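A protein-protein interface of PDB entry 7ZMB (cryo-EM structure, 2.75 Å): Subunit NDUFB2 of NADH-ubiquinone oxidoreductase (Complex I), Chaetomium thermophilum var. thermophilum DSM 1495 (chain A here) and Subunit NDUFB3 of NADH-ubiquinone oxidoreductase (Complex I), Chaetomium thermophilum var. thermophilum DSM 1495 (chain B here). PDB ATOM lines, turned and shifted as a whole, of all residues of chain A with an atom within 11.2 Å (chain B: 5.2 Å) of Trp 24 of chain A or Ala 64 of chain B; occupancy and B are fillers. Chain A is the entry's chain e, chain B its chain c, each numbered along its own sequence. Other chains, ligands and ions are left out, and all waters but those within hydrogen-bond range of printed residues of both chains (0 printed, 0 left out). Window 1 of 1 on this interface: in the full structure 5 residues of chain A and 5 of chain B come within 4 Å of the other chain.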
ATOM      1  N   ALA A  16      12.688   0.779 -40.339  1.00  0.00           N
ATOM      2  CA  ALA A  16      13.791   0.419 -39.454  1.00  0.00           C
ATOM      3  C   ALA A  16      14.114   1.554 -38.493  1.00  0.00           C
ATOM      4  O   ALA A  16      14.171   1.355 -37.274  1.00  0.00           O
ATOM      5  CB  ALA A  16      15.024   0.048 -40.279  1.00  0.00           C
ATOM      6  N   THR A  17      14.322   2.759 -39.024  1.00  0.00           N
ATOM      7  CA  THR A  17      14.607   3.900 -38.163  1.00  0.00           C
ATOM      8  C   THR A  17      13.356   4.388 -37.449  1.00  0.00           C
ATOM      9  O   THR A  17      13.440   4.845 -36.305  1.00  0.00           O
ATOM     10  CB  THR A  17      15.228   5.034 -38.976  1.00  0.00           C
ATOM     11  OG1 THR A  17      14.305   5.462 -39.985  1.00  0.00           O
ATOM     12  CG2 THR A  17      16.516   4.570 -39.636  1.00  0.00           C
ATOM     13  N   GLY A  18      12.194   4.303 -38.101  1.00  0.00           N
ATOM     14  CA  GLY A  18      10.971   4.781 -37.477  1.00  0.00           C
ATOM     15  C   GLY A  18      10.643   4.035 -36.199  1.00  0.00           C
ATOM     16  O   GLY A  18      10.322   4.641 -35.174  1.00  0.00           O
ATOM     17  N   LEU A  19      10.773   2.741 -36.187  1.00  0.00           N
ATOM     18  CA  LEU A  19      10.573   1.981 -34.928  1.00  0.00           C
ATOM     19  C   LEU A  19      11.772   2.292 -34.034  1.00  0.00           C
ATOM     20  O   LEU A  19      11.596   2.412 -32.815  1.00  0.00           O
ATOM     21  CB  LEU A  19      10.497   0.491 -35.254  1.00  0.00           C
ATOM     22  CG  LEU A  19       9.275   0.063 -36.065  1.00  0.00           C
ATOM     23  CD1 LEU A  19       9.404  -1.383 -36.512  1.00  0.00           C
ATOM     24  CD2 LEU A  19       7.998   0.265 -35.266  1.00  0.00           C
ATOM     25  N   GLY A  20      12.980   2.377 -34.647  1.00  0.00           N
ATOM     26  CA  GLY A  20      14.120   2.794 -33.855  1.00  0.00           C
ATOM     27  C   GLY A  20      13.997   4.198 -33.307  1.00  0.00           C
ATOM     28  O   GLY A  20      14.640   4.518 -32.302  1.00  0.00           O
ATOM     29  N   ALA A  21      13.192   5.046 -33.949  1.00  0.00           N
ATOM     30  CA  ALA A  21      12.919   6.380 -33.429  1.00  0.00           C
ATOM     31  C   ALA A  21      11.824   6.363 -32.372  1.00  0.00           C
ATOM     32  O   ALA A  21      11.881   7.137 -31.411  1.00  0.00           O
ATOM     33  CB  ALA A  21      12.527   7.325 -34.567  1.00  0.00           C
ATOM     34  N   SER A  22      10.819   5.500 -32.539  1.00  0.00           N
ATOM     35  CA  SER A  22       9.820   5.327 -31.491  1.00  0.00           C
ATOM     36  C   SER A  22      10.472   4.818 -30.214  1.00  0.00           C
ATOM     37  O   SER A  22      10.208   5.327 -29.119  1.00  0.00           O
ATOM     38  CB  SER A  22       8.727   4.370 -31.964  1.00  0.00           C
ATOM     39  OG  SER A  22       9.259   3.085 -32.229  1.00  0.00           O
ATOM     40  N   MET A  23      11.337   3.816 -30.340  1.00  0.00           N
ATOM     41  CA  MET A  23      12.201   3.441 -29.236  1.00  0.00           C
ATOM     42  C   MET A  23      13.321   4.470 -29.102  1.00  0.00           C
ATOM     43  O   MET A  23      13.507   5.334 -29.963  1.00  0.00           O
ATOM     44  CB  MET A  23      12.769   2.037 -29.456  1.00  0.00           C
ATOM     45  CG  MET A  23      13.253   1.346 -28.192  1.00  0.00           C
ATOM     46  SD  MET A  23      14.315  -0.061 -28.552  1.00  0.00           S
ATOM     47  CE  MET A  23      15.911   0.739 -28.633  1.00  0.00           C
ATOM     48  N   TRP A  24      14.042   4.399 -27.984  1.00  0.00           N
ATOM     49  CA  TRP A  24      15.088   5.337 -27.584  1.00  0.00           C
ATOM     50  C   TRP A  24      14.528   6.724 -27.297  1.00  0.00           C
ATOM     51  O   TRP A  24      15.276   7.598 -26.845  1.00  0.00           O
ATOM     52  CB  TRP A  24      16.208   5.461 -28.628  1.00  0.00           C
ATOM     53  CG  TRP A  24      17.194   4.335 -28.614  1.00  0.00           C
ATOM     54  CD1 TRP A  24      17.592   3.590 -29.682  1.00  0.00           C
ATOM     55  CD2 TRP A  24      17.914   3.831 -27.482  1.00  0.00           C
ATOM     56  NE1 TRP A  24      18.512   2.650 -29.288  1.00  0.00           N
ATOM     57  CE2 TRP A  24      18.725   2.778 -27.940  1.00  0.00           C
ATOM     58  CE3 TRP A  24      17.949   4.168 -26.126  1.00  0.00           C
ATOM     59  CZ2 TRP A  24      19.561   2.058 -27.094  1.00  0.00           C
ATOM     60  CZ3 TRP A  24      18.779   3.453 -25.288  1.00  0.00           C
ATOM     61  CH2 TRP A  24      19.575   2.410 -25.774  1.00  0.00           C
ATOM     62  N   PHE A  25      13.241   6.950 -27.540  1.00  0.00           N
ATOM     63  CA  PHE A  25      12.537   8.145 -27.108  1.00  0.00           C
ATOM     64  C   PHE A  25      11.537   7.858 -26.006  1.00  0.00           C
ATOM     65  O   PHE A  25      11.299   8.719 -25.161  1.00  0.00           O
ATOM     66  CB  PHE A  25      11.806   8.794 -28.291  1.00  0.00           C
ATOM     67  CG  PHE A  25      10.940   9.960 -27.908  1.00  0.00           C
ATOM     68  CD1 PHE A  25      11.490  11.214 -27.707  1.00  0.00           C
ATOM     69  CD2 PHE A  25       9.571   9.804 -27.759  1.00  0.00           C
ATOM     70  CE1 PHE A  25      10.694  12.288 -27.358  1.00  0.00           C
ATOM     71  CE2 PHE A  25       8.770  10.874 -27.409  1.00  0.00           C
ATOM     72  CZ  PHE A  25       9.332  12.117 -27.209  1.00  0.00           C
ATOM     73  N   TRP A  26      10.959   6.656 -25.998  1.00  0.00           N
ATOM     74  CA  TRP A  26      10.095   6.237 -24.906  1.00  0.00           C
ATOM     75  C   TRP A  26      10.858   6.088 -23.599  1.00  0.00           C
ATOM     76  O   TRP A  26      10.247   6.153 -22.528  1.00  0.00           O
ATOM     77  CB  TRP A  26       9.412   4.918 -25.267  1.00  0.00           C
ATOM     78  CG  TRP A  26       8.542   4.371 -24.187  1.00  0.00           C
ATOM     79  CD1 TRP A  26       8.856   3.380 -23.307  1.00  0.00           C
ATOM     80  CD2 TRP A  26       7.208   4.779 -23.874  1.00  0.00           C
ATOM     81  NE1 TRP A  26       7.800   3.148 -22.461  1.00  0.00           N
ATOM     82  CE2 TRP A  26       6.776   3.995 -22.789  1.00  0.00           C
ATOM     83  CE3 TRP A  26       6.337   5.735 -24.404  1.00  0.00           C
ATOM     84  CZ2 TRP A  26       5.512   4.135 -22.225  1.00  0.00           C
ATOM     85  CZ3 TRP A  26       5.083   5.871 -23.844  1.00  0.00           C
ATOM     86  CH2 TRP A  26       4.681   5.075 -22.767  1.00  0.00           C
ATOM     87  N   ILE A  27      12.176   5.901 -23.658  1.00  0.00           N
ATOM     88  CA  ILE A  27      12.961   5.719 -22.441  1.00  0.00           C
ATOM     89  C   ILE A  27      13.212   7.057 -21.757  1.00  0.00           C
ATOM     90  O   ILE A  27      12.837   7.259 -20.596  1.00  0.00           O
ATOM     91  CB  ILE A  27      14.282   4.997 -22.757  1.00  0.00           C
ATOM     92  CG1 ILE A  27      14.002   3.632 -23.386  1.00  0.00           C
ATOM     93  CG2 ILE A  27      15.115   4.841 -21.498  1.00  0.00           C
ATOM     94  CD1 ILE A  27      15.150   3.099 -24.205  1.00  0.00           C
ATOM     95  N   PHE A  28      13.853   7.988 -22.469  1.00  0.00           N
ATOM     96  CA  PHE A  28      14.162   9.287 -21.881  1.00  0.00           C
ATOM     97  C   PHE A  28      12.901  10.041 -21.492  1.00  0.00           C
ATOM     98  O   PHE A  28      12.870  10.706 -20.450  1.00  0.00           O
ATOM     99  CB  PHE A  28      14.995  10.120 -22.852  1.00  0.00           C
ATOM    100  CG  PHE A  28      16.368   9.572 -23.100  1.00  0.00           C
ATOM    101  CD1 PHE A  28      17.390   9.799 -22.195  1.00  0.00           C
ATOM    102  CD2 PHE A  28      16.641   8.841 -24.242  1.00  0.00           C
ATOM    103  CE1 PHE A  28      18.658   9.300 -22.420  1.00  0.00           C
ATOM    104  CE2 PHE A  28      17.906   8.340 -24.475  1.00  0.00           C
ATOM    105  CZ  PHE A  28      18.916   8.570 -23.562  1.00  0.00           C
ATOM    106  N   TYR A  29      11.857   9.957 -22.317  1.00  0.00           N
ATOM    107  CA  TYR A  29      10.582  10.569 -21.966  1.00  0.00           C
ATOM    108  C   TYR A  29      10.036   9.968 -20.679  1.00  0.00           C
ATOM    109  O   TYR A  29       9.478  10.681 -19.838  1.00  0.00           O
ATOM    110  CB  TYR A  29       9.603  10.406 -23.133  1.00  0.00           C
ATOM    111  CG  TYR A  29       8.200  10.955 -22.944  1.00  0.00           C
ATOM    112  CD1 TYR A  29       7.305  10.373 -22.055  1.00  0.00           C
ATOM    113  CD2 TYR A  29       7.772  12.059 -23.669  1.00  0.00           C
ATOM    114  CE1 TYR A  29       6.028  10.871 -21.898  1.00  0.00           C
ATOM    115  CE2 TYR A  29       6.499  12.568 -23.514  1.00  0.00           C
ATOM    116  CZ  TYR A  29       5.631  11.972 -22.625  1.00  0.00           C
ATOM    117  OH  TYR A  29       4.361  12.473 -22.467  1.00  0.00           O
ATOM    118  N   ARG A  30      10.189   8.654 -20.508  1.00  0.00           N
ATOM    119  CA  ARG A  30       9.722   8.015 -19.284  1.00  0.00           C
ATOM    120  C   ARG A  30      10.718   8.192 -18.145  1.00  0.00           C
ATOM    121  O   ARG A  30      10.318   8.344 -16.985  1.00  0.00           O
ATOM    122  CB  ARG A  30       9.441   6.537 -19.547  1.00  0.00           C
ATOM    123  CG  ARG A  30       8.968   5.768 -18.338  1.00  0.00           C
ATOM    124  CD  ARG A  30       7.624   6.310 -17.920  1.00  0.00           C
ATOM    125  NE  ARG A  30       6.616   6.068 -18.942  1.00  0.00           N
ATOM    126  CZ  ARG A  30       5.418   6.639 -18.948  1.00  0.00           C
ATOM    127  NH1 ARG A  30       5.075   7.477 -17.981  1.00  0.00           N
ATOM    128  NH2 ARG A  30       4.566   6.379 -19.926  1.00  0.00           N
ATOM    129  N   ALA A  31      12.017   8.184 -18.455  1.00  0.00           N
ATOM    130  CA  ALA A  31      13.021   8.446 -17.431  1.00  0.00           C
ATOM    131  C   ALA A  31      12.922   9.860 -16.880  1.00  0.00           C
ATOM    132  O   ALA A  31      13.422  10.121 -15.781  1.00  0.00           O
ATOM    133  CB  ALA A  31      14.422   8.202 -17.987  1.00  0.00           C
ATOM    134  N   LYS A  32      12.294  10.777 -17.618  1.00  0.00           N
ATOM    135  CA  LYS A  32      12.108  12.133 -17.114  1.00  0.00           C
ATOM    136  C   LYS A  32      11.145  12.161 -15.934  1.00  0.00           C
ATOM    137  O   LYS A  32      11.281  13.009 -15.045  1.00  0.00           O
ATOM    138  CB  LYS A  32      11.603  13.040 -18.236  1.00  0.00           C
ATOM    139  CG  LYS A  32      11.474  14.512 -17.863  1.00  0.00           C
ATOM    140  CD  LYS A  32      12.835  15.176 -17.726  1.00  0.00           C
ATOM    141  CE  LYS A  32      12.701  16.673 -17.492  1.00  0.00           C
ATOM    142  NZ  LYS A  32      12.301  17.399 -18.730  1.00  0.00           N
ATOM    143  N   LEU B  58      22.564   1.651 -33.184  1.00  0.00           N
ATOM    144  CA  LEU B  58      21.309   2.161 -32.635  1.00  0.00           C
ATOM    145  C   LEU B  58      20.664   3.029 -33.704  1.00  0.00           C
ATOM    146  O   LEU B  58      21.047   4.201 -33.870  1.00  0.00           O
ATOM    147  CB  LEU B  58      21.550   2.958 -31.356  1.00  0.00           C
ATOM    148  CG  LEU B  58      22.399   2.275 -30.282  1.00  0.00           C
ATOM    149  CD1 LEU B  58      22.394   3.098 -29.006  1.00  0.00           C
ATOM    150  CD2 LEU B  58      21.899   0.866 -30.012  1.00  0.00           C
ATOM    151  N   GLY B  60      17.598   4.645 -34.503  1.00  0.00           N
ATOM    152  CA  GLY B  60      16.907   5.883 -34.228  1.00  0.00           C
ATOM    153  C   GLY B  60      17.415   6.668 -33.040  1.00  0.00           C
ATOM    154  O   GLY B  60      16.792   7.667 -32.669  1.00  0.00           O
ATOM    155  N   PHE B  61      18.526   6.250 -32.432  1.00  0.00           N
ATOM    156  CA  PHE B  61      19.009   6.925 -31.230  1.00  0.00           C
ATOM    157  C   PHE B  61      19.384   8.373 -31.516  1.00  0.00           C
ATOM    158  O   PHE B  61      19.061   9.270 -30.730  1.00  0.00           O
ATOM    159  CB  PHE B  61      20.199   6.168 -30.648  1.00  0.00           C
ATOM    160  CG  PHE B  61      20.735   6.770 -29.385  1.00  0.00           C
ATOM    161  CD1 PHE B  61      20.065   6.608 -28.187  1.00  0.00           C
ATOM    162  CD2 PHE B  61      21.913   7.494 -29.395  1.00  0.00           C
ATOM    163  CE1 PHE B  61      20.555   7.159 -27.023  1.00  0.00           C
ATOM    164  CE2 PHE B  61      22.410   8.048 -28.234  1.00  0.00           C
ATOM    165  CZ  PHE B  61      21.730   7.880 -27.046  1.00  0.00           C
ATOM    166  N   GLY B  62      20.066   8.621 -32.634  1.00  0.00           N
ATOM    167  CA  GLY B  62      20.470   9.981 -32.949  1.00  0.00           C
ATOM    168  C   GLY B  62      19.291  10.902 -33.195  1.00  0.00           C
ATOM    169  O   GLY B  62      19.268  12.039 -32.720  1.00  0.00           O
ATOM    170  N   ILE B  63      18.293  10.421 -33.937  1.00  0.00           N
ATOM    171  CA  ILE B  63      17.135  11.250 -34.254  1.00  0.00           C
ATOM    172  C   ILE B  63      16.296  11.498 -33.006  1.00  0.00           C
ATOM    173  O   ILE B  63      15.773  12.600 -32.802  1.00  0.00           O
ATOM    174  CB  ILE B  63      16.303  10.604 -35.380  1.00  0.00           C
ATOM    175  CG1 ILE B  63      17.115  10.504 -36.677  1.00  0.00           C
ATOM    176  CG2 ILE B  63      15.026  11.391 -35.624  1.00  0.00           C
ATOM    177  CD1 ILE B  63      17.924   9.229 -36.822  1.00  0.00           C
ATOM    178  N   ALA B  64      16.159  10.483 -32.150  1.00  0.00           N
ATOM    179  CA  ALA B  64      15.285  10.600 -30.987  1.00  0.00           C
ATOM    180  C   ALA B  64      15.766  11.683 -30.028  1.00  0.00           C
ATOM    181  O   ALA B  64      14.955  12.433 -29.473  1.00  0.00           O
ATOM    182  CB  ALA B  64      15.188   9.256 -30.268  1.00  0.00           C
ATOM    183  N   THR B  65      17.080  11.777 -29.815  1.00  0.00           N
ATOM    184  CA  THR B  65      17.606  12.761 -28.874  1.00  0.00           C
ATOM    185  C   THR B  65      17.286  14.181 -29.319  1.00  0.00           C
ATOM    186  O   THR B  65      17.013  15.053 -28.485  1.00  0.00           O
ATOM    187  CB  THR B  65      19.115  12.584 -28.707  1.00  0.00           C
ATOM    188  OG1 THR B  65      19.764  12.789 -29.967  1.00  0.00           O
ATOM    189  CG2 THR B  65      19.436  11.191 -28.188  1.00  0.00           C
ATOM    190  N   VAL B  66      17.316  14.434 -30.628  1.00  0.00           N
ATOM    191  CA  VAL B  66      17.000  15.767 -31.136  1.00  0.00           C
ATOM    192  C   VAL B  66      15.574  16.147 -30.762  1.00  0.00           C
ATOM    193  O   VAL B  66      15.309  17.264 -30.302  1.00  0.00           O
ATOM    194  CB  VAL B  66      17.221  15.828 -32.657  1.00  0.00           C
ATOM    195  CG1 VAL B  66      16.815  17.189 -33.198  1.00  0.00           C
ATOM    196  CG2 VAL B  66      18.671  15.526 -32.992  1.00  0.00           C
ATOM    197  N   ALA B  67      14.633  15.219 -30.950  1.00  0.00           N
ATOM    198  CA  ALA B  67      13.255  15.477 -30.553  1.00  0.00           C
ATOM    199  C   ALA B  67      13.123  15.558 -29.038  1.00  0.00           C
ATOM    200  O   ALA B  67      12.311  16.333 -28.520  1.00  0.00           O
ATOM    201  CB  ALA B  67      12.333  14.398 -31.117  1.00  0.00           C
ATOM    202  N   PHE B  68      13.906  14.758 -28.310  1.00  0.00           N
ATOM    203  CA  PHE B  68      13.837  14.778 -26.852  1.00  0.00           C
ATOM    204  C   PHE B  68      14.219  16.145 -26.299  1.00  0.00           C
ATOM    205  O   PHE B  68      13.543  16.673 -25.408  1.00  0.00           O
ATOM    206  CB  PHE B  68      14.746  13.695 -26.270  1.00  0.00           C
ATOM    207  CG  PHE B  68      14.767  13.662 -24.768  1.00  0.00           C
ATOM    208  CD1 PHE B  68      13.602  13.841 -24.039  1.00  0.00           C
ATOM    209  CD2 PHE B  68      15.955  13.473 -24.084  1.00  0.00           C
ATOM    210  CE1 PHE B  68      13.621  13.818 -22.659  1.00  0.00           C
ATOM    211  CE2 PHE B  68      15.981  13.451 -22.704  1.00  0.00           C
ATOM    212  CZ  PHE B  68      14.812  13.623 -21.990  1.00  0.00           C
ATOM    213  N   THR B  69      15.299  16.736 -26.815  1.00  0.00           N
ATOM    214  CA  THR B  69      15.711  18.054 -26.344  1.00  0.00           C
ATOM    215  C   THR B  69      14.670  19.109 -26.690  1.00  0.00           C
ATOM    216  O   THR B  69      14.450  20.051 -25.918  1.00  0.00           O
ATOM    217  CB  THR B  69      17.070  18.426 -26.938  1.00  0.00           C
ATOM    218  OG1 THR B  69      16.971  18.478 -28.365  1.00  0.00           O
ATOM    219  CG2 THR B  69      18.124  17.405 -26.538  1.00  0.00           C
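Among the printed residues, pairs that only touch across the chains: Gly 20 of chain A with Gly 60 of chain B (3.3 Å), Phe 28 of chain A with Phe 68 of chain B (3.5 Å), Trp 24 of chain A with Leu 58 of chain B (3.6 Å), Trp 24 of chain A with Phe 61 of chain B (3.6 Å), Trp 24 of chain A with Ala 64 of chain B (3.8 Å), Ala 21 of chain A with Gly 60 of chain B (3.8 Å), Phe 28 of chain A with Phe 61 of chain B (3.9 Å) and Phe 25 of chain A with Ala 64 of chain B (3.9 Å).
Printed residues of chain B within 4 Å of Gly 20 of chain A: Gly 60.
Trp 24 of chain A touches three residues of chain B.
Of the printed residues of chain B, Phe 28 of chain A touches Phe 61 and Phe 68.
Of chain A, only Gly 20 (3.3 Å) and Ala 21 (3.8 Å) come within 4 Å of Gly 60 of chain B.
Gly 62 of chain B touches none of the printed residues of chain A.
No residue of chain A comes within 4 Å of Ile 63 of chain B.
No residue of chain A comes within 4 Å of Thr 65 of chain B.
Ala 67 of chain B touches none of the printed residues of chain A.
Printed residues of chain A that touch a printed residue of chain B: Gly 20, Ala 21, Trp 24, Phe 25 and Phe 28.
Hydrophobic or aromatic side chains of chain A within 4 Å of the printed part of chain B: Trp 24, Phe 25 and Phe 28.
Hydrophobic or aromatic side chains of chain B within 4 Å of the printed part of chain A: Leu 58, Phe 61, Ala 64 and Phe 68.
Along chain B the printed residues that touch a printed residue of chain A span positions 58 to 68.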
